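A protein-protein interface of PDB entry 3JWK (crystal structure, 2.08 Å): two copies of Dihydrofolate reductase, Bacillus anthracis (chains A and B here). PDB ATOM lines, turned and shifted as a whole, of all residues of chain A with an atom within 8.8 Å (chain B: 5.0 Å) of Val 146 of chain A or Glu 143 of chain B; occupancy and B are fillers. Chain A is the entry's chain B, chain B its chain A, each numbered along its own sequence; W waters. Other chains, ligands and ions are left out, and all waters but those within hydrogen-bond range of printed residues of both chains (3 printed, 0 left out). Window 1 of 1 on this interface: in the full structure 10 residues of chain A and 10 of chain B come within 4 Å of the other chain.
NZ of Lys 142 of chain B is in salt-bridge range of OE2 of Glu 143 of chain A (3.3 Å). The backbone NH (N) of Trp 141 of chain B is in hydrogen-bond range of the backbone carbonyl oxygen (O) of Val 144 of chain A. The side-chain hydroxyl (OH) of Tyr 164 of chain B lies within hydrogen-bond range of the side-chain carboxylate (OE1) of Glu 147 of chain A. The side-chain carboxylate (OE2) of Glu 143 of chain B sits at hydrogen-bond distance from the backbone NH (N) of Lys 148 of chain A, at 2.8 Å. The backbone carbonyl oxygen (O) of Val 146 of chain A is in hydrogen-bond range of the backbone NH (N) of Glu 143 of chain B, 3.0 Å away.
OE1 of Glu 143 of chain A sits at hydrogen-bond distance from ND1 of His 162 of chain A (2.7 Å). The backbone carbonyl oxygen of Phe 145 of chain A sits at hydrogen-bond distance from the backbone NH of Val 163 of chain A (2.9 Å). The backbone NH of Val 144 of chain A is in hydrogen-bond range of the backbone carbonyl oxygen of Val 163 of chain A (2.8 Å). The backbone carbonyl oxygen (O) of Glu 147 of chain A lies within hydrogen-bond range of the backbone NH (N) of Tyr 161 of chain A, 2.8 Å away. OE1 of Glu 143 of chain B sits at hydrogen-bond distance from ND1 of His 162 of chain B (2.7 Å).
Among the printed residues, merely in contact across the chains: Phe 145 of chain A with Trp 141 of chain B (3.2 Å), Val 146 of chain A with Trp 141 of chain B (3.97 Å), Val 146 of chain A with Lys 142 of chain B (3.8 Å), Glu 147 of chain A with Glu 143 of chain B (3.6 Å) and Lys 148 of chain A with Val 146 of chain B (3.9 Å).
Val 146 of chain A touches just these residues of chain B: Trp 141 (3.97 Å), Lys 142 (3.8 Å) and Glu 143 (3.0 Å). Printed residues of chain B within 4 Å of Glu 147 of chain A: Glu 143 (3.6 Å) and Tyr 164 (2.5 Å). Val 163 of chain A touches none of the printed residues of chain B. Of the printed residues of chain A, Lys 142 of chain B touches Glu 143 (3.3 Å) and Val 146 (3.8 Å). Glu 143 of chain B touches just these residues of chain A: Val 146 (3.0 Å), Glu 147 (3.6 Å) and Lys 148 (2.8 Å). The nearest printed residue of chain A that does not touch Val 146 of chain B is Tyr 160 of chain A (5.8 Å).
Of the 9 printed residues of chain B, 5 touch a printed residue of chain A. Hydrophobic or aromatic side chains of chain B that line the printed part of chain A: Val 146 and Tyr 164. Along chain B the printed residues that touch a printed residue of chain A span positions 141 to 164. Of the 18 printed residues of chain A, 6 touch a printed residue of chain B. Hydrophobic or aromatic side chains of chain A within 4 Å of the printed part of chain B: Phe 145 and Val 146. Among the printed residues, Asp or Glu carboxylates within 4 Å of a Lys or Arg side-chain nitrogen of the other chain: Glu 143 of chain A with Lys 142 of chain B.
Val 146 of chain A touches Glu 143 of chain B, but with the chains exchanged Glu 143 of chain A does not touch Val 146 of chain B (13.2 Å). 7 positions are printed for both chains.
Water W2 lies within hydrogen-bond range of the side-chain amino group (NZ) of Lys 142 of chain B (2.6 Å) and the backbone carbonyl oxygen (O) of Glu 143 of chain A (3.1 Å). Water W3 lies within hydrogen-bond range of O of Lys 148 of chain A (2.6 Å), OE1 of Glu 143 of chain B (2.7 Å) and ND1 of His 162 of chain B (3.3 Å). Water W1 bridges the side-chain carboxylate of Glu 147 of chain A (2.7 Å) and the side-chain hydroxyl of Tyr 164 of chain B (3.4 Å).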
ATOM      1  N   TYR A  37       9.098  12.157 -12.565  1.00  0.00           N
ATOM      2  CA  TYR A  37       9.157  11.216 -13.684  1.00  0.00           C
ATOM      3  C   TYR A  37       8.014  11.437 -14.667  1.00  0.00           C
ATOM      4  O   TYR A  37       8.218  11.371 -15.867  1.00  0.00           O
ATOM      5  CB  TYR A  37       9.096   9.788 -13.165  1.00  0.00           C
ATOM      6  CG  TYR A  37       8.968   8.714 -14.226  1.00  0.00           C
ATOM      7  CD1 TYR A  37      10.103   8.202 -14.858  1.00  0.00           C
ATOM      8  CD2 TYR A  37       7.717   8.187 -14.580  1.00  0.00           C
ATOM      9  CE1 TYR A  37      10.004   7.206 -15.817  1.00  0.00           C
ATOM     10  CE2 TYR A  37       7.613   7.169 -15.542  1.00  0.00           C
ATOM     11  CZ  TYR A  37       8.762   6.693 -16.149  1.00  0.00           C
ATOM     12  OH  TYR A  37       8.697   5.696 -17.098  1.00  0.00           O
ATOM     13  N   ILE A 120       3.748   2.278 -16.619  1.00  0.00           N
ATOM     14  CA  ILE A 120       3.104   1.966 -15.341  1.00  0.00           C
ATOM     15  C   ILE A 120       4.096   2.058 -14.207  1.00  0.00           C
ATOM     16  O   ILE A 120       5.123   1.379 -14.214  1.00  0.00           O
ATOM     17  CB  ILE A 120       2.546   0.515 -15.248  1.00  0.00           C
ATOM     18  CG1 ILE A 120       1.750   0.118 -16.467  1.00  0.00           C
ATOM     19  CG2 ILE A 120       1.657   0.347 -13.991  1.00  0.00           C
ATOM     20  CD1 ILE A 120       0.718  -1.015 -16.166  1.00  0.00           C
ATOM     21  N   LYS A 122       4.505   0.875 -10.535  1.00  0.00           N
ATOM     22  CA  LYS A 122       3.942  -0.144  -9.674  1.00  0.00           C
ATOM     23  C   LYS A 122       4.391   0.132  -8.244  1.00  0.00           C
ATOM     24  O   LYS A 122       5.587   0.100  -7.949  1.00  0.00           O
ATOM     25  CB  LYS A 122       4.357  -1.548 -10.147  1.00  0.00           C
ATOM     26  CG  LYS A 122       3.855  -1.906 -11.553  1.00  0.00           C
ATOM     27  CD  LYS A 122       3.958  -3.396 -11.822  1.00  0.00           C
ATOM     28  CE  LYS A 122       3.528  -3.745 -13.247  1.00  0.00           C
ATOM     29  NZ  LYS A 122       3.695  -5.225 -13.485  1.00  0.00           N
ATOM     30  N   HIS A 124       4.502  -0.870  -4.337  1.00  0.00           N
ATOM     31  CA  HIS A 124       4.525  -2.113  -3.557  1.00  0.00           C
ATOM     32  C   HIS A 124       3.909  -1.879  -2.187  1.00  0.00           C
ATOM     33  O   HIS A 124       4.586  -1.977  -1.161  1.00  0.00           O
ATOM     34  CB  HIS A 124       5.978  -2.654  -3.438  1.00  0.00           C
ATOM     35  CG  HIS A 124       6.591  -3.063  -4.745  1.00  0.00           C
ATOM     36  ND1 HIS A 124       7.617  -3.980  -4.833  1.00  0.00           N
ATOM     37  CD2 HIS A 124       6.317  -2.688  -6.019  1.00  0.00           C
ATOM     38  CE1 HIS A 124       7.942  -4.157  -6.103  1.00  0.00           C
ATOM     39  NE2 HIS A 124       7.169  -3.382  -6.845  1.00  0.00           N
ATOM     40  N   GLU A 143       8.193  -5.904 -21.854  1.00  0.00           N
ATOM     41  CA  GLU A 143       8.792  -4.901 -20.979  1.00  0.00           C
ATOM     42  C   GLU A 143      10.061  -4.364 -21.638  1.00  0.00           C
ATOM     43  O   GLU A 143      10.976  -5.127 -21.917  1.00  0.00           O
ATOM     44  CB  GLU A 143       9.114  -5.500 -19.613  1.00  0.00           C
ATOM     45  CG  GLU A 143       9.489  -4.451 -18.577  1.00  0.00           C
ATOM     46  CD  GLU A 143       9.933  -5.063 -17.268  1.00  0.00           C
ATOM     47  OE1 GLU A 143       9.369  -4.698 -16.215  1.00  0.00           O
ATOM     48  OE2 GLU A 143      10.840  -5.921 -17.285  1.00  0.00           O
ATOM     49  N   VAL A 144      10.098  -3.053 -21.881  1.00  0.00           N
ATOM     50  CA  VAL A 144      11.205  -2.413 -22.575  1.00  0.00           C
ATOM     51  C   VAL A 144      12.047  -1.529 -21.625  1.00  0.00           C
ATOM     52  O   VAL A 144      13.106  -1.029 -22.004  1.00  0.00           O
ATOM     53  CB  VAL A 144      10.706  -1.620 -23.835  1.00  0.00           C
ATOM     54  CG1 VAL A 144      10.003  -2.555 -24.818  1.00  0.00           C
ATOM     55  CG2 VAL A 144       9.790  -0.436 -23.441  1.00  0.00           C
ATOM     56  N   PHE A 145      11.583  -1.385 -20.385  1.00  0.00           N
ATOM     57  CA  PHE A 145      12.294  -0.603 -19.374  1.00  0.00           C
ATOM     58  C   PHE A 145      11.727  -0.885 -17.991  1.00  0.00           C
ATOM     59  O   PHE A 145      10.516  -1.070 -17.818  1.00  0.00           O
ATOM     60  CB  PHE A 145      12.232   0.896 -19.698  1.00  0.00           C
ATOM     61  CG  PHE A 145      12.945   1.769 -18.693  1.00  0.00           C
ATOM     62  CD1 PHE A 145      14.336   1.882 -18.708  1.00  0.00           C
ATOM     63  CD2 PHE A 145      12.221   2.461 -17.725  1.00  0.00           C
ATOM     64  CE1 PHE A 145      14.994   2.688 -17.775  1.00  0.00           C
ATOM     65  CE2 PHE A 145      12.862   3.277 -16.794  1.00  0.00           C
ATOM     66  CZ  PHE A 145      14.253   3.392 -16.820  1.00  0.00           C
ATOM     67  N   VAL A 146      12.628  -0.937 -17.018  1.00  0.00           N
ATOM     68  CA  VAL A 146      12.276  -1.071 -15.607  1.00  0.00           C
ATOM     69  C   VAL A 146      13.391  -0.440 -14.788  1.00  0.00           C
ATOM     70  O   VAL A 146      14.577  -0.630 -15.093  1.00  0.00           O
ATOM     71  CB  VAL A 146      12.024  -2.560 -15.179  1.00  0.00           C
ATOM     72  CG1 VAL A 146      13.286  -3.425 -15.360  1.00  0.00           C
ATOM     73  CG2 VAL A 146      11.504  -2.644 -13.725  1.00  0.00           C
ATOM     74  N   GLU A 147      13.013   0.356 -13.791  1.00  0.00           N
ATOM     75  CA  GLU A 147      13.965   0.855 -12.796  1.00  0.00           C
ATOM     76  C   GLU A 147      13.246   1.151 -11.490  1.00  0.00           C
ATOM     77  O   GLU A 147      12.056   1.480 -11.487  1.00  0.00           O
ATOM     78  CB  GLU A 147      14.801   2.055 -13.288  1.00  0.00           C
ATOM     79  CG  GLU A 147      14.085   3.390 -13.334  1.00  0.00           C
ATOM     80  CD  GLU A 147      15.012   4.594 -13.527  1.00  0.00           C
ATOM     81  OE1 GLU A 147      16.152   4.451 -14.024  1.00  0.00           O
ATOM     82  OE2 GLU A 147      14.578   5.711 -13.183  1.00  0.00           O
ATOM     83  N   LYS A 148      13.981   1.001 -10.391  1.00  0.00           N
ATOM     84  CA  LYS A 148      13.449   1.220  -9.067  1.00  0.00           C
ATOM     85  C   LYS A 148      13.280   2.717  -8.847  1.00  0.00           C
ATOM     86  O   LYS A 148      14.157   3.519  -9.218  1.00  0.00           O
ATOM     87  CB  LYS A 148      14.396   0.605  -8.024  1.00  0.00           C
ATOM     88  CG  LYS A 148      13.864   0.628  -6.586  1.00  0.00           C
ATOM     89  CD  LYS A 148      14.757  -0.173  -5.657  1.00  0.00           C
ATOM     90  CE  LYS A 148      14.150  -0.283  -4.258  1.00  0.00           C
ATOM     91  NZ  LYS A 148      13.886   1.087  -3.725  1.00  0.00           N
ATOM     92  N   GLY A 149      12.148   3.095  -8.262  1.00  0.00           N
ATOM     93  CA  GLY A 149      11.896   4.492  -7.917  1.00  0.00           C
ATOM     94  C   GLY A 149      12.649   4.892  -6.659  1.00  0.00           C
ATOM     95  O   GLY A 149      13.137   4.038  -5.909  1.00  0.00           O
ATOM     96  N   LEU A 150      12.725   6.197  -6.420  1.00  0.00           N
ATOM     97  CA  LEU A 150      13.417   6.742  -5.263  1.00  0.00           C
ATOM     98  C   LEU A 150      12.554   6.608  -4.010  1.00  0.00           C
ATOM     99  O   LEU A 150      11.467   7.190  -3.931  1.00  0.00           O
ATOM    100  CB  LEU A 150      13.720   8.228  -5.497  1.00  0.00           C
ATOM    101  CG  LEU A 150      14.864   8.962  -4.775  1.00  0.00           C
ATOM    102  CD1 LEU A 150      14.431  10.374  -4.393  1.00  0.00           C
ATOM    103  CD2 LEU A 150      15.488   8.243  -3.573  1.00  0.00           C
ATOM    104  N   TYR A 159       8.540   1.413  -4.978  1.00  0.00           N
ATOM    105  CA  TYR A 159       7.869   1.440  -6.271  1.00  0.00           C
ATOM    106  C   TYR A 159       8.869   1.334  -7.434  1.00  0.00           C
ATOM    107  O   TYR A 159      10.063   1.654  -7.280  1.00  0.00           O
ATOM    108  CB  TYR A 159       6.972   2.688  -6.417  1.00  0.00           C
ATOM    109  CG  TYR A 159       7.708   4.004  -6.298  1.00  0.00           C
ATOM    110  CD1 TYR A 159       8.004   4.761  -7.435  1.00  0.00           C
ATOM    111  CD2 TYR A 159       8.131   4.482  -5.053  1.00  0.00           C
ATOM    112  CE1 TYR A 159       8.688   5.955  -7.331  1.00  0.00           C
ATOM    113  CE2 TYR A 159       8.834   5.680  -4.942  1.00  0.00           C
ATOM    114  CZ  TYR A 159       9.110   6.405  -6.083  1.00  0.00           C
ATOM    115  OH  TYR A 159       9.786   7.597  -5.989  1.00  0.00           O
ATOM    116  N   TYR A 160       8.375   0.890  -8.588  1.00  0.00           N
ATOM    117  CA  TYR A 160       9.212   0.688  -9.777  1.00  0.00           C
ATOM    118  C   TYR A 160       8.520   1.285 -10.988  1.00  0.00           C
ATOM    119  O   TYR A 160       7.298   1.221 -11.101  1.00  0.00           O
ATOM    120  CB  TYR A 160       9.463  -0.817 -10.029  1.00  0.00           C
ATOM    121  CG  TYR A 160      10.447  -1.469  -9.073  1.00  0.00           C
ATOM    122  CD1 TYR A 160      10.086  -1.747  -7.749  1.00  0.00           C
ATOM    123  CD2 TYR A 160      11.740  -1.814  -9.496  1.00  0.00           C
ATOM    124  CE1 TYR A 160      10.991  -2.340  -6.864  1.00  0.00           C
ATOM    125  CE2 TYR A 160      12.656  -2.396  -8.617  1.00  0.00           C
ATOM    126  CZ  TYR A 160      12.269  -2.658  -7.304  1.00  0.00           C
ATOM    127  OH  TYR A 160      13.157  -3.236  -6.427  1.00  0.00           O
ATOM    128  N   TYR A 161       9.314   1.863 -11.889  1.00  0.00           N
ATOM    129  CA  TYR A 161       8.820   2.347 -13.173  1.00  0.00           C
ATOM    130  C   TYR A 161       8.951   1.183 -14.147  1.00  0.00           C
ATOM    131  O   TYR A 161      10.014   0.566 -14.223  1.00  0.00           O
ATOM    132  CB  TYR A 161       9.664   3.532 -13.668  1.00  0.00           C
ATOM    133  CG  TYR A 161       9.668   4.720 -12.727  1.00  0.00           C
ATOM    134  CD1 TYR A 161      10.841   5.112 -12.065  1.00  0.00           C
ATOM    135  CD2 TYR A 161       8.497   5.462 -12.500  1.00  0.00           C
ATOM    136  CE1 TYR A 161      10.855   6.205 -11.210  1.00  0.00           C
ATOM    137  CE2 TYR A 161       8.497   6.566 -11.629  1.00  0.00           C
ATOM    138  CZ  TYR A 161       9.686   6.919 -10.983  1.00  0.00           C
ATOM    139  OH  TYR A 161       9.705   7.997 -10.127  1.00  0.00           O
ATOM    140  N   HIS A 162       7.859   0.853 -14.833  1.00  0.00           N
ATOM    141  CA  HIS A 162       7.853  -0.155 -15.890  1.00  0.00           C
ATOM    142  C   HIS A 162       7.332   0.478 -17.172  1.00  0.00           C
ATOM    143  O   HIS A 162       6.439   1.317 -17.135  1.00  0.00           O
ATOM    144  CB  HIS A 162       6.952  -1.341 -15.529  1.00  0.00           C
ATOM    145  CG  HIS A 162       7.365  -2.071 -14.287  1.00  0.00           C
ATOM    146  ND1 HIS A 162       8.106  -3.231 -14.317  1.00  0.00           N
ATOM    147  CD2 HIS A 162       7.134  -1.808 -12.978  1.00  0.00           C
ATOM    148  CE1 HIS A 162       8.310  -3.656 -13.080  1.00  0.00           C
ATOM    149  NE2 HIS A 162       7.740  -2.804 -12.248  1.00  0.00           N
ATOM    150  N   VAL A 163       7.910   0.080 -18.302  1.00  0.00           N
ATOM    151  CA  VAL A 163       7.408   0.477 -19.607  1.00  0.00           C
ATOM    152  C   VAL A 163       7.245  -0.772 -20.463  1.00  0.00           C
ATOM    153  O   VAL A 163       8.169  -1.588 -20.567  1.00  0.00           O
ATOM    154  CB  VAL A 163       8.325   1.505 -20.322  1.00  0.00           C
ATOM    155  CG1 VAL A 163       7.651   2.018 -21.579  1.00  0.00           C
ATOM    156  CG2 VAL A 163       8.648   2.696 -19.394  1.00  0.00           C
ATOM    157  N   TYR A 164       6.062  -0.916 -21.055  1.00  0.00           N
ATOM    158  CA  TYR A 164       5.716  -2.058 -21.901  1.00  0.00           C
ATOM    159  C   TYR A 164       5.331  -1.537 -23.277  1.00  0.00           C
ATOM    160  O   TYR A 164       4.682  -0.490 -23.398  1.00  0.00           O
ATOM    161  CB  TYR A 164       4.525  -2.832 -21.321  1.00  0.00           C
ATOM    162  CG  TYR A 164       4.746  -3.375 -19.934  1.00  0.00           C
ATOM    163  CD1 TYR A 164       5.252  -4.663 -19.744  1.00  0.00           C
ATOM    164  CD2 TYR A 164       4.456  -2.597 -18.806  1.00  0.00           C
ATOM    165  CE1 TYR A 164       5.469  -5.162 -18.468  1.00  0.00           C
ATOM    166  CE2 TYR A 164       4.665  -3.086 -17.532  1.00  0.00           C
ATOM    167  CZ  TYR A 164       5.175  -4.361 -17.365  1.00  0.00           C
ATOM    168  OH  TYR A 164       5.386  -4.846 -16.097  1.00  0.00           O
ATOM    169  N   TRP B 141      16.413  -0.817 -22.281  1.00  0.00           N
ATOM    170  CA  TRP B 141      17.389  -1.036 -21.227  1.00  0.00           C
ATOM    171  C   TRP B 141      16.664  -1.380 -19.939  1.00  0.00           C
ATOM    172  O   TRP B 141      15.583  -0.858 -19.669  1.00  0.00           O
ATOM    173  CB  TRP B 141      18.225   0.206 -21.004  1.00  0.00           C
ATOM    174  CG  TRP B 141      19.185   0.493 -22.098  1.00  0.00           C
ATOM    175  CD1 TRP B 141      18.890   0.879 -23.373  1.00  0.00           C
ATOM    176  CD2 TRP B 141      20.610   0.450 -22.007  1.00  0.00           C
ATOM    177  NE1 TRP B 141      20.051   1.071 -24.093  1.00  0.00           N
ATOM    178  CE2 TRP B 141      21.123   0.808 -23.276  1.00  0.00           C
ATOM    179  CE3 TRP B 141      21.504   0.134 -20.981  1.00  0.00           C
ATOM    180  CZ2 TRP B 141      22.493   0.872 -23.539  1.00  0.00           C
ATOM    181  CZ3 TRP B 141      22.867   0.195 -21.244  1.00  0.00           C
ATOM    182  CH2 TRP B 141      23.344   0.565 -22.514  1.00  0.00           C
ATOM    183  N   LYS B 142      17.260  -2.265 -19.149  1.00  0.00           N
ATOM    184  CA  LYS B 142      16.725  -2.600 -17.834  1.00  0.00           C
ATOM    185  C   LYS B 142      17.767  -2.395 -16.744  1.00  0.00           C
ATOM    186  O   LYS B 142      18.929  -2.778 -16.901  1.00  0.00           O
ATOM    187  CB  LYS B 142      16.217  -4.043 -17.772  1.00  0.00           C
ATOM    188  CG  LYS B 142      15.056  -4.351 -18.716  1.00  0.00           C
ATOM    189  CD  LYS B 142      14.512  -5.754 -18.462  1.00  0.00           C
ATOM    190  CE  LYS B 142      13.340  -6.032 -19.384  1.00  0.00           C
ATOM    191  NZ  LYS B 142      12.918  -7.446 -19.265  1.00  0.00           N
ATOM    192  N   GLU B 143      17.329  -1.804 -15.637  1.00  0.00           N
ATOM    193  CA  GLU B 143      18.145  -1.710 -14.436  1.00  0.00           C
ATOM    194  C   GLU B 143      18.311  -3.106 -13.848  1.00  0.00           C
ATOM    195  O   GLU B 143      17.314  -3.777 -13.532  1.00  0.00           O
ATOM    196  CB  GLU B 143      17.482  -0.799 -13.407  1.00  0.00           C
ATOM    197  CG  GLU B 143      18.378  -0.410 -12.236  1.00  0.00           C
ATOM    198  CD  GLU B 143      17.695   0.550 -11.288  1.00  0.00           C
ATOM    199  OE1 GLU B 143      18.165   1.693 -11.201  1.00  0.00           O
ATOM    200  OE2 GLU B 143      16.696   0.171 -10.630  1.00  0.00           O
ATOM    201  N   VAL B 144      19.563  -3.539 -13.709  1.00  0.00           N
ATOM    202  CA  VAL B 144      19.863  -4.879 -13.184  1.00  0.00           C
ATOM    203  C   VAL B 144      20.500  -4.799 -11.806  1.00  0.00           C
ATOM    204  O   VAL B 144      20.682  -5.814 -11.140  1.00  0.00           O
ATOM    205  CB  VAL B 144      20.773  -5.734 -14.117  1.00  0.00           C
ATOM    206  CG1 VAL B 144      20.097  -5.980 -15.460  1.00  0.00           C
ATOM    207  CG2 VAL B 144      22.148  -5.091 -14.300  1.00  0.00           C
ATOM    208  N   PHE B 145      20.837  -3.590 -11.380  1.00  0.00           N
ATOM    209  CA  PHE B 145      21.425  -3.396 -10.069  1.00  0.00           C
ATOM    210  C   PHE B 145      21.216  -1.959  -9.600  1.00  0.00           C
ATOM    211  O   PHE B 145      21.346  -1.014 -10.379  1.00  0.00           O
ATOM    212  CB  PHE B 145      22.927  -3.750 -10.078  1.00  0.00           C
ATOM    213  CG  PHE B 145      23.614  -3.533  -8.759  1.00  0.00           C
ATOM    214  CD1 PHE B 145      23.492  -4.471  -7.731  1.00  0.00           C
ATOM    215  CD2 PHE B 145      24.385  -2.386  -8.539  1.00  0.00           C
ATOM    216  CE1 PHE B 145      24.128  -4.271  -6.494  1.00  0.00           C
ATOM    217  CE2 PHE B 145      25.015  -2.169  -7.304  1.00  0.00           C
ATOM    218  CZ  PHE B 145      24.891  -3.115  -6.285  1.00  0.00           C
ATOM    219  N   VAL B 146      20.893  -1.815  -8.319  1.00  0.00           N
ATOM    220  CA  VAL B 146      20.806  -0.500  -7.676  1.00  0.00           C
ATOM    221  C   VAL B 146      21.122  -0.638  -6.188  1.00  0.00           C
ATOM    222  O   VAL B 146      20.667  -1.570  -5.529  1.00  0.00           O
ATOM    223  CB  VAL B 146      19.436   0.211  -7.944  1.00  0.00           C
ATOM    224  CG1 VAL B 146      18.245  -0.589  -7.351  1.00  0.00           C
ATOM    225  CG2 VAL B 146      19.443   1.654  -7.448  1.00  0.00           C
ATOM    226  N   HIS B 162      23.822   2.606  -9.985  1.00  0.00           N
ATOM    227  CA  HIS B 162      22.873   1.972 -10.886  1.00  0.00           C
ATOM    228  C   HIS B 162      23.640   1.231 -11.967  1.00  0.00           C
ATOM    229  O   HIS B 162      24.682   1.707 -12.436  1.00  0.00           O
ATOM    230  CB  HIS B 162      21.966   2.998 -11.576  1.00  0.00           C
ATOM    231  CG  HIS B 162      21.196   3.873 -10.638  1.00  0.00           C
ATOM    232  ND1 HIS B 162      19.872   3.653 -10.327  1.00  0.00           N
ATOM    233  CD2 HIS B 162      21.561   4.987  -9.957  1.00  0.00           C
ATOM    234  CE1 HIS B 162      19.455   4.590  -9.494  1.00  0.00           C
ATOM    235  NE2 HIS B 162      20.464   5.408  -9.248  1.00  0.00           N
ATOM    236  N   VAL B 163      23.128   0.070 -12.359  1.00  0.00           N
ATOM    237  CA  VAL B 163      23.646  -0.635 -13.532  1.00  0.00           C
ATOM    238  C   VAL B 163      22.476  -0.976 -14.450  1.00  0.00           C
ATOM    239  O   VAL B 163      21.494  -1.571 -14.007  1.00  0.00           O
ATOM    240  CB  VAL B 163      24.445  -1.909 -13.129  1.00  0.00           C
ATOM    241  CG1 VAL B 163      25.088  -2.570 -14.350  1.00  0.00           C
ATOM    242  CG2 VAL B 163      25.509  -1.572 -12.091  1.00  0.00           C
ATOM    243  N   TYR B 164      22.570  -0.559 -15.713  1.00  0.00           N
ATOM    244  CA  TYR B 164      21.587  -0.891 -16.730  1.00  0.00           C
ATOM    245  C   TYR B 164      22.241  -1.760 -17.805  1.00  0.00           C
ATOM    246  O   TYR B 164      23.407  -1.556 -18.139  1.00  0.00           O
ATOM    247  CB  TYR B 164      21.018   0.376 -17.380  1.00  0.00           C
ATOM    248  CG  TYR B 164      20.384   1.383 -16.421  1.00  0.00           C
ATOM    249  CD1 TYR B 164      19.007   1.390 -16.198  1.00  0.00           C
ATOM    250  CD2 TYR B 164      21.158   2.333 -15.765  1.00  0.00           C
ATOM    251  CE1 TYR B 164      18.417   2.314 -15.325  1.00  0.00           C
ATOM    252  CE2 TYR B 164      20.578   3.265 -14.882  1.00  0.00           C
ATOM    253  CZ  TYR B 164      19.206   3.244 -14.675  1.00  0.00           C
ATOM    254  OH  TYR B 164      18.623   4.157 -13.818  1.00  0.00           O
HETATM  255  O   HOH W   1      16.838   6.137 -15.971  1.00  0.00           O
HETATM  256  O   HOH W   2      11.427  -8.109 -21.258  1.00  0.00           O
HETATM  257  O   HOH W   3      16.629   3.563 -10.108  1.00  0.00           O
